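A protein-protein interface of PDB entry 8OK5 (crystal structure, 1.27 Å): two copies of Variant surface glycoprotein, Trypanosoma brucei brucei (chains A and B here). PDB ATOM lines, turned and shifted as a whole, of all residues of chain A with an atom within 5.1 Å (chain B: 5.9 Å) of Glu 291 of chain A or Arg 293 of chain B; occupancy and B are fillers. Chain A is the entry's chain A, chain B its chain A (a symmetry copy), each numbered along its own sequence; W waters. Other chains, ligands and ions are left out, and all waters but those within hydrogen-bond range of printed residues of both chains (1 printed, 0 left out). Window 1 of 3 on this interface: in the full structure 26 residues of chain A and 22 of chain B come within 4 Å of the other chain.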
ATOM      1  N   ALA A 287      16.371   9.823  33.476  1.00  0.00           N
ATOM      2  CA  ALA A 287      17.092  11.082  33.598  1.00  0.00           C
ATOM      3  C   ALA A 287      16.444  12.171  32.751  1.00  0.00           C
ATOM      4  O   ALA A 287      16.271  13.303  33.221  1.00  0.00           O
ATOM      5  CB  ALA A 287      18.552  10.892  33.224  1.00  0.00           C
ATOM      6  N   ALA A 288      16.042  11.846  31.521  1.00  0.00           N
ATOM      7  CA  ALA A 288      15.410  12.843  30.658  1.00  0.00           C
ATOM      8  C   ALA A 288      14.178  13.442  31.326  1.00  0.00           C
ATOM      9  O   ALA A 288      13.961  14.666  31.297  1.00  0.00           O
ATOM     10  CB  ALA A 288      15.020  12.208  29.325  1.00  0.00           C
ATOM     11  N   ALA A 289      13.362  12.604  31.960  1.00  0.00           N
ATOM     12  CA  ALA A 289      12.137  13.087  32.588  1.00  0.00           C
ATOM     13  C   ALA A 289      12.442  14.058  33.725  1.00  0.00           C
ATOM     14  O   ALA A 289      11.786  15.098  33.846  1.00  0.00           O
ATOM     15  CB  ALA A 289      11.301  11.904  33.075  1.00  0.00           C
ATOM     16  N   ILE A 290      13.438  13.747  34.556  1.00  0.00           N
ATOM     17  CA  ILE A 290      13.827  14.670  35.621  1.00  0.00           C
ATOM     18  C   ILE A 290      14.397  15.951  35.039  1.00  0.00           C
ATOM     19  O   ILE A 290      14.128  17.048  35.539  1.00  0.00           O
ATOM     20  CB  ILE A 290      14.844  14.011  36.569  1.00  0.00           C
ATOM     21  CG1 ILE A 290      14.288  12.747  37.237  1.00  0.00           C
ATOM     22  CG2 ILE A 290      15.323  15.020  37.630  1.00  0.00           C
ATOM     23  CD1 ILE A 290      13.019  12.914  37.978  1.00  0.00           C
ATOM     24  N   GLU A 291      15.228  15.841  34.010  1.00  0.00           N
ATOM     25  CA  GLU A 291      15.851  17.010  33.425  1.00  0.00           C
ATOM     26  C   GLU A 291      14.782  17.974  32.927  1.00  0.00           C
ATOM     27  O   GLU A 291      14.866  19.182  33.139  1.00  0.00           O
ATOM     28  CB  GLU A 291      16.789  16.609  32.280  1.00  0.00           C
ATOM     29  CG  GLU A 291      17.306  17.818  31.486  1.00  0.00           C
ATOM     30  CD  GLU A 291      16.400  18.169  30.287  1.00  0.00           C
ATOM     31  OE1 GLU A 291      15.819  17.218  29.699  1.00  0.00           O
ATOM     32  OE2 GLU A 291      16.221  19.381  29.956  1.00  0.00           O
ATOM     33  N   GLY A 292      13.785  17.452  32.206  1.00  0.00           N
ATOM     34  CA  GLY A 292      12.751  18.322  31.680  1.00  0.00           C
ATOM     35  C   GLY A 292      11.984  19.021  32.789  1.00  0.00           C
ATOM     36  O   GLY A 292      11.621  20.199  32.671  1.00  0.00           O
ATOM     37  N   ARG A 293      11.726  18.315  33.893  1.00  0.00           N
ATOM     38  CA  ARG A 293      10.935  18.880  34.973  1.00  0.00           C
ATOM     39  C   ARG A 293      11.716  19.960  35.706  1.00  0.00           C
ATOM     40  O   ARG A 293      11.149  20.987  36.066  1.00  0.00           O
ATOM     41  CB  ARG A 293      10.492  17.761  35.924  1.00  0.00           C
ATOM     42  CG  ARG A 293       9.375  16.871  35.378  1.00  0.00           C
ATOM     43  CD  ARG A 293       9.091  15.700  36.352  1.00  0.00           C
ATOM     44  NE  ARG A 293       7.775  15.077  36.138  1.00  0.00           N
ATOM     45  CZ  ARG A 293       7.507  14.291  35.112  1.00  0.00           C
ATOM     46  NH1 ARG A 293       8.410  14.029  34.194  1.00  0.00           N
ATOM     47  NH2 ARG A 293       6.306  13.727  35.006  1.00  0.00           N
ATOM     48  N   LEU A 294      13.014  19.761  35.924  1.00  0.00           N
ATOM     49  CA  LEU A 294      13.824  20.797  36.541  1.00  0.00           C
ATOM     50  C   LEU A 294      13.914  22.043  35.656  1.00  0.00           C
ATOM     51  O   LEU A 294      13.712  23.169  36.147  1.00  0.00           O
ATOM     52  CB  LEU A 294      15.241  20.279  36.778  1.00  0.00           C
ATOM     53  CG  LEU A 294      15.384  19.396  38.014  1.00  0.00           C
ATOM     54  CD1 LEU A 294      16.674  18.629  37.959  1.00  0.00           C
ATOM     55  CD2 LEU A 294      15.303  20.240  39.289  1.00  0.00           C
ATOM     56  N   THR A 295      14.181  21.875  34.353  1.00  0.00           N
ATOM     57  CA  THR A 295      14.284  23.013  33.444  1.00  0.00           C
ATOM     58  C   THR A 295      12.994  23.805  33.440  1.00  0.00           C
ATOM     59  O   THR A 295      13.006  25.042  33.344  1.00  0.00           O
ATOM     60  CB  THR A 295      14.570  22.525  32.036  1.00  0.00           C
ATOM     61  OG1 THR A 295      15.851  21.888  32.008  1.00  0.00           O
ATOM     62  CG2 THR A 295      14.587  23.670  31.045  1.00  0.00           C
ATOM     63  N   ALA A 296      11.859  23.107  33.527  1.00  0.00           N
ATOM     64  CA  ALA A 296      10.559  23.781  33.483  1.00  0.00           C
ATOM     65  C   ALA A 296      10.377  24.709  34.670  1.00  0.00           C
ATOM     66  O   ALA A 296       9.687  25.719  34.543  1.00  0.00           O
ATOM     67  CB  ALA A 296       9.443  22.732  33.449  1.00  0.00           C
ATOM     68  N   ARG A 354      18.706  12.896  38.785  1.00  0.00           N
ATOM     69  CA  ARG A 354      18.945  12.806  37.346  1.00  0.00           C
ATOM     70  C   ARG A 354      20.312  12.203  37.047  1.00  0.00           C
ATOM     71  O   ARG A 354      20.444  11.357  36.145  1.00  0.00           O
ATOM     72  CB  ARG A 354      18.835  14.197  36.706  1.00  0.00           C
ATOM     73  CG  ARG A 354      19.201  14.209  35.210  1.00  0.00           C
ATOM     74  CD  ARG A 354      19.479  15.596  34.670  1.00  0.00           C
ATOM     75  NE  ARG A 354      20.605  16.250  35.334  1.00  0.00           N
ATOM     76  CZ  ARG A 354      21.868  16.206  34.928  1.00  0.00           C
ATOM     77  NH1 ARG A 354      22.228  15.522  33.856  1.00  0.00           N
ATOM     78  NH2 ARG A 354      22.796  16.890  35.605  1.00  0.00           N
ATOM     79  N   ALA B  36      11.068  29.888  27.310  1.00  0.00           N
ATOM     80  CA  ALA B  36      11.365  29.044  26.165  1.00  0.00           C
ATOM     81  C   ALA B  36      12.618  29.519  25.455  1.00  0.00           C
ATOM     82  O   ALA B  36      13.494  28.712  25.118  1.00  0.00           O
ATOM     83  CB  ALA B  36      10.174  29.014  25.199  1.00  0.00           C
ATOM     84  N   GLY B  39      15.787  28.845  27.393  1.00  0.00           N
ATOM     85  CA  GLY B  39      16.190  27.471  27.282  1.00  0.00           C
ATOM     86  C   GLY B  39      17.046  27.226  26.074  1.00  0.00           C
ATOM     87  O   GLY B  39      17.747  26.206  26.031  1.00  0.00           O
ATOM     88  N   ILE B  40      16.993  28.103  25.086  1.00  0.00           N
ATOM     89  CA  ILE B  40      17.930  28.060  23.961  1.00  0.00           C
ATOM     90  C   ILE B  40      19.231  28.781  24.303  1.00  0.00           C
ATOM     91  O   ILE B  40      20.319  28.238  24.079  1.00  0.00           O
ATOM     92  CB  ILE B  40      17.286  28.685  22.709  1.00  0.00           C
ATOM     93  CG1 ILE B  40      15.942  28.009  22.399  1.00  0.00           C
ATOM     94  CG2 ILE B  40      18.242  28.642  21.511  1.00  0.00           C
ATOM     95  CD1 ILE B  40      15.985  26.545  22.160  1.00  0.00           C
ATOM     96  N   GLU B  42      20.668  29.434  27.014  1.00  0.00           N
ATOM     97  CA  GLU B  42      21.530  28.835  28.029  1.00  0.00           C
ATOM     98  C   GLU B  42      22.420  27.739  27.463  1.00  0.00           C
ATOM     99  O   GLU B  42      23.392  27.377  28.108  1.00  0.00           O
ATOM    100  CB  GLU B  42      20.702  28.320  29.196  1.00  0.00           C
ATOM    101  CG  GLU B  42      19.882  27.110  28.932  1.00  0.00           C
ATOM    102  CD  GLU B  42      19.040  26.722  30.132  1.00  0.00           C
ATOM    103  OE1 GLU B  42      19.284  27.287  31.213  1.00  0.00           O
ATOM    104  OE2 GLU B  42      18.119  25.887  30.002  1.00  0.00           O
ATOM    105  N   LEU B  43      22.103  27.227  26.286  1.00  0.00           N
ATOM    106  CA  LEU B  43      22.921  26.195  25.657  1.00  0.00           C
ATOM    107  C   LEU B  43      24.187  26.736  25.052  1.00  0.00           C
ATOM    108  O   LEU B  43      25.075  25.939  24.745  1.00  0.00           O
ATOM    109  CB  LEU B  43      22.156  25.542  24.512  1.00  0.00           C
ATOM    110  CG  LEU B  43      20.873  24.831  24.895  1.00  0.00           C
ATOM    111  CD1 LEU B  43      20.131  24.379  23.626  1.00  0.00           C
ATOM    112  CD2 LEU B  43      21.086  23.672  25.790  1.00  0.00           C
ATOM    113  N   THR B 283      24.697  22.493  30.664  1.00  0.00           N
ATOM    114  CA  THR B 283      23.615  21.610  30.253  1.00  0.00           C
ATOM    115  C   THR B 283      24.233  20.345  29.672  1.00  0.00           C
ATOM    116  O   THR B 283      25.186  20.421  28.895  1.00  0.00           O
ATOM    117  CB  THR B 283      22.714  22.263  29.194  1.00  0.00           C
ATOM    118  OG1 THR B 283      22.099  23.453  29.716  1.00  0.00           O
ATOM    119  CG2 THR B 283      21.596  21.311  28.747  1.00  0.00           C
ATOM    120  N   SER B 286      21.999  16.140  25.169  1.00  0.00           N
ATOM    121  CA  SER B 286      21.333  14.932  24.729  1.00  0.00           C
ATOM    122  C   SER B 286      20.347  15.337  23.647  1.00  0.00           C
ATOM    123  O   SER B 286      19.846  16.456  23.650  1.00  0.00           O
ATOM    124  CB  SER B 286      20.575  14.252  25.871  1.00  0.00           C
ATOM    125  OG  SER B 286      19.696  15.136  26.546  1.00  0.00           O
ATOM    126  N   ALA B 288      17.326  14.307  23.296  1.00  0.00           N
ATOM    127  CA  ALA B 288      16.038  14.566  23.938  1.00  0.00           C
ATOM    128  C   ALA B 288      15.977  15.986  24.487  1.00  0.00           C
ATOM    129  O   ALA B 288      14.969  16.696  24.328  1.00  0.00           O
ATOM    130  CB  ALA B 288      15.803  13.563  25.064  1.00  0.00           C
ATOM    131  N   ALA B 289      17.056  16.439  25.119  1.00  0.00           N
ATOM    132  CA  ALA B 289      17.067  17.771  25.716  1.00  0.00           C
ATOM    133  C   ALA B 289      16.917  18.855  24.653  1.00  0.00           C
ATOM    134  O   ALA B 289      16.161  19.814  24.846  1.00  0.00           O
ATOM    135  CB  ALA B 289      18.344  17.964  26.533  1.00  0.00           C
ATOM    136  N   ILE B 290      17.614  18.718  23.524  1.00  0.00           N
ATOM    137  CA  ILE B 290      17.458  19.685  22.438  1.00  0.00           C
ATOM    138  C   ILE B 290      16.056  19.622  21.860  1.00  0.00           C
ATOM    139  O   ILE B 290      15.458  20.652  21.537  1.00  0.00           O
ATOM    140  CB  ILE B 290      18.506  19.441  21.337  1.00  0.00           C
ATOM    141  CG1 ILE B 290      19.943  19.565  21.860  1.00  0.00           C
ATOM    142  CG2 ILE B 290      18.275  20.400  20.153  1.00  0.00           C
ATOM    143  CD1 ILE B 290      20.279  20.838  22.531  1.00  0.00           C
ATOM    144  N   GLU B 291      15.524  18.420  21.671  1.00  0.00           N
ATOM    145  CA  GLU B 291      14.210  18.271  21.082  1.00  0.00           C
ATOM    146  C   GLU B 291      13.174  18.997  21.930  1.00  0.00           C
ATOM    147  O   GLU B 291      12.307  19.698  21.411  1.00  0.00           O
ATOM    148  CB  GLU B 291      13.844  16.788  20.943  1.00  0.00           C
ATOM    149  CG  GLU B 291      12.382  16.574  20.527  1.00  0.00           C
ATOM    150  CD  GLU B 291      11.437  16.435  21.740  1.00  0.00           C
ATOM    151  OE1 GLU B 291      11.896  15.880  22.773  1.00  0.00           O
ATOM    152  OE2 GLU B 291      10.264  16.914  21.692  1.00  0.00           O
ATOM    153  N   GLY B 292      13.222  18.794  23.250  1.00  0.00           N
ATOM    154  CA  GLY B 292      12.245  19.437  24.108  1.00  0.00           C
ATOM    155  C   GLY B 292      12.341  20.951  24.035  1.00  0.00           C
ATOM    156  O   GLY B 292      11.323  21.657  24.054  1.00  0.00           O
ATOM    157  N   ARG B 293      13.562  21.483  23.945  1.00  0.00           N
ATOM    158  CA  ARG B 293      13.751  22.924  23.944  1.00  0.00           C
ATOM    159  C   ARG B 293      13.262  23.531  22.638  1.00  0.00           C
ATOM    160  O   ARG B 293      12.650  24.595  22.650  1.00  0.00           O
ATOM    161  CB  ARG B 293      15.228  23.248  24.199  1.00  0.00           C
ATOM    162  CG  ARG B 293      15.681  23.044  25.644  1.00  0.00           C
ATOM    163  CD  ARG B 293      17.209  23.271  25.771  1.00  0.00           C
ATOM    164  NE  ARG B 293      17.642  23.532  27.152  1.00  0.00           N
ATOM    165  CZ  ARG B 293      17.704  22.595  28.078  1.00  0.00           C
ATOM    166  NH1 ARG B 293      17.356  21.353  27.822  1.00  0.00           N
ATOM    167  NH2 ARG B 293      18.147  22.896  29.297  1.00  0.00           N
ATOM    168  N   LEU B 294      13.503  22.873  21.507  1.00  0.00           N
ATOM    169  CA  LEU B 294      12.983  23.364  20.243  1.00  0.00           C
ATOM    170  C   LEU B 294      11.452  23.341  20.217  1.00  0.00           C
ATOM    171  O   LEU B 294      10.822  24.343  19.834  1.00  0.00           O
ATOM    172  CB  LEU B 294      13.491  22.494  19.095  1.00  0.00           C
ATOM    173  CG  LEU B 294      14.919  22.809  18.659  1.00  0.00           C
ATOM    174  CD1 LEU B 294      15.468  21.687  17.826  1.00  0.00           C
ATOM    175  CD2 LEU B 294      14.966  24.133  17.892  1.00  0.00           C
ATOM    176  N   THR B 295      10.830  22.233  20.645  1.00  0.00           N
ATOM    177  CA  THR B 295       9.373  22.132  20.651  1.00  0.00           C
ATOM    178  C   THR B 295       8.770  23.227  21.504  1.00  0.00           C
ATOM    179  O   THR B 295       7.704  23.773  21.182  1.00  0.00           O
ATOM    180  CB  THR B 295       8.951  20.783  21.203  1.00  0.00           C
ATOM    181  OG1 THR B 295       9.410  19.749  20.327  1.00  0.00           O
ATOM    182  CG2 THR B 295       7.445  20.678  21.317  1.00  0.00           C
ATOM    183  N   ALA B 296       9.432  23.556  22.617  1.00  0.00           N
ATOM    184  CA  ALA B 296       8.903  24.570  23.532  1.00  0.00           C
ATOM    185  C   ALA B 296       8.835  25.932  22.866  1.00  0.00           C
ATOM    186  O   ALA B 296       7.961  26.727  23.212  1.00  0.00           O
ATOM    187  CB  ALA B 296       9.780  24.632  24.786  1.00  0.00           C
ATOM    188  N   VAL B 297       9.744  26.247  21.952  1.00  0.00           N
ATOM    189  CA  VAL B 297       9.642  27.455  21.170  1.00  0.00           C
ATOM    190  C   VAL B 297       8.661  27.276  20.021  1.00  0.00           C
ATOM    191  O   VAL B 297       7.798  28.147  19.795  1.00  0.00           O
ATOM    192  CB  VAL B 297      11.031  27.884  20.646  1.00  0.00           C
ATOM    193  CG1 VAL B 297      10.902  29.059  19.679  1.00  0.00           C
ATOM    194  CG2 VAL B 297      11.952  28.182  21.789  1.00  0.00           C
ATOM    195  N   GLY B 298       8.812  26.175  19.281  1.00  0.00           N
ATOM    196  CA  GLY B 298       8.081  26.037  18.022  1.00  0.00           C
ATOM    197  C   GLY B 298       6.578  26.069  18.182  1.00  0.00           C
ATOM    198  O   GLY B 298       5.879  26.669  17.372  1.00  0.00           O
ATOM    199  N   LEU B 350      19.696  24.342  15.098  1.00  0.00           N
ATOM    200  CA  LEU B 350      19.675  23.634  16.371  1.00  0.00           C
ATOM    201  C   LEU B 350      19.159  22.208  16.205  1.00  0.00           C
ATOM    202  O   LEU B 350      19.663  21.278  16.858  1.00  0.00           O
ATOM    203  CB  LEU B 350      18.871  24.442  17.385  1.00  0.00           C
ATOM    204  CG  LEU B 350      19.040  24.018  18.841  1.00  0.00           C
ATOM    205  CD1 LEU B 350      20.507  24.166  19.290  1.00  0.00           C
ATOM    206  CD2 LEU B 350      18.104  24.858  19.721  1.00  0.00           C
HETATM  207  O   HOH W   1      17.985  23.950  32.139  1.00  0.00           O
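The side-chain carboxylate of Glu 291 of chain A lies within salt-bridge range of the guanidinium group of Arg 293 of chain B (3.1 Å).
The guanidinium group of Arg 293 of chain B is in hydrogen-bond range of the backbone carbonyl oxygen of Gly 39 of chain B, 2.9 Å away.
OG1 of Thr 295 of chain A lies within hydrogen-bond range of O of Glu 291 of chain A.
The guanidinium group of Arg 293 of chain B is in salt-bridge range of the side-chain carboxylate of Glu 42 of chain B, 3.1 Å away.
Among the printed residues, pairs that only touch across the chains: Thr 295 of chain A with Arg 293 of chain B (3.7 Å).
Glu 291 of chain A touches one residue of chain B.
Of chain A, only Glu 291 (3.1 Å) and Thr 295 (3.7 Å) come within 4 Å of Arg 293 of chain B.
Of the printed residues of chain B, Thr 295 of chain A touches Arg 293.
Arg 293 of chain A touches none of the printed residues of chain B.
The nearest printed residue of chain B that does not touch Thr 295 of chain A is Glu 42 of chain B (4.3 Å).
Among the printed residues, 2 pairs touch across the chains.
Among the printed residues, Asp or Glu carboxylates within 4 Å of a Lys or Arg side-chain nitrogen of the other chain: Glu 291 of chain A with Arg 293 of chain B (3.1 Å).
Glu 291 of chain A touches Arg 293 of chain B, but with the chains exchanged Arg 293 of chain A does not touch Glu 291 of chain B (11.4 Å).
Thr 295 of chain A touches Arg 293 of chain B, but with the chains exchanged Arg 293 of chain A does not touch Thr 295 of chain B (13.2 Å).
Positions printed for both chains: 288, 289, 290, 291, 292, 293, 294, 295 and 296.
Water W1 lies within hydrogen-bond range of OE2 of Glu 42 of chain B (2.9 Å), OG1 of Thr 295 of chain A (3.0 Å) and NH2 of Arg 293 of chain B (3.0 Å).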
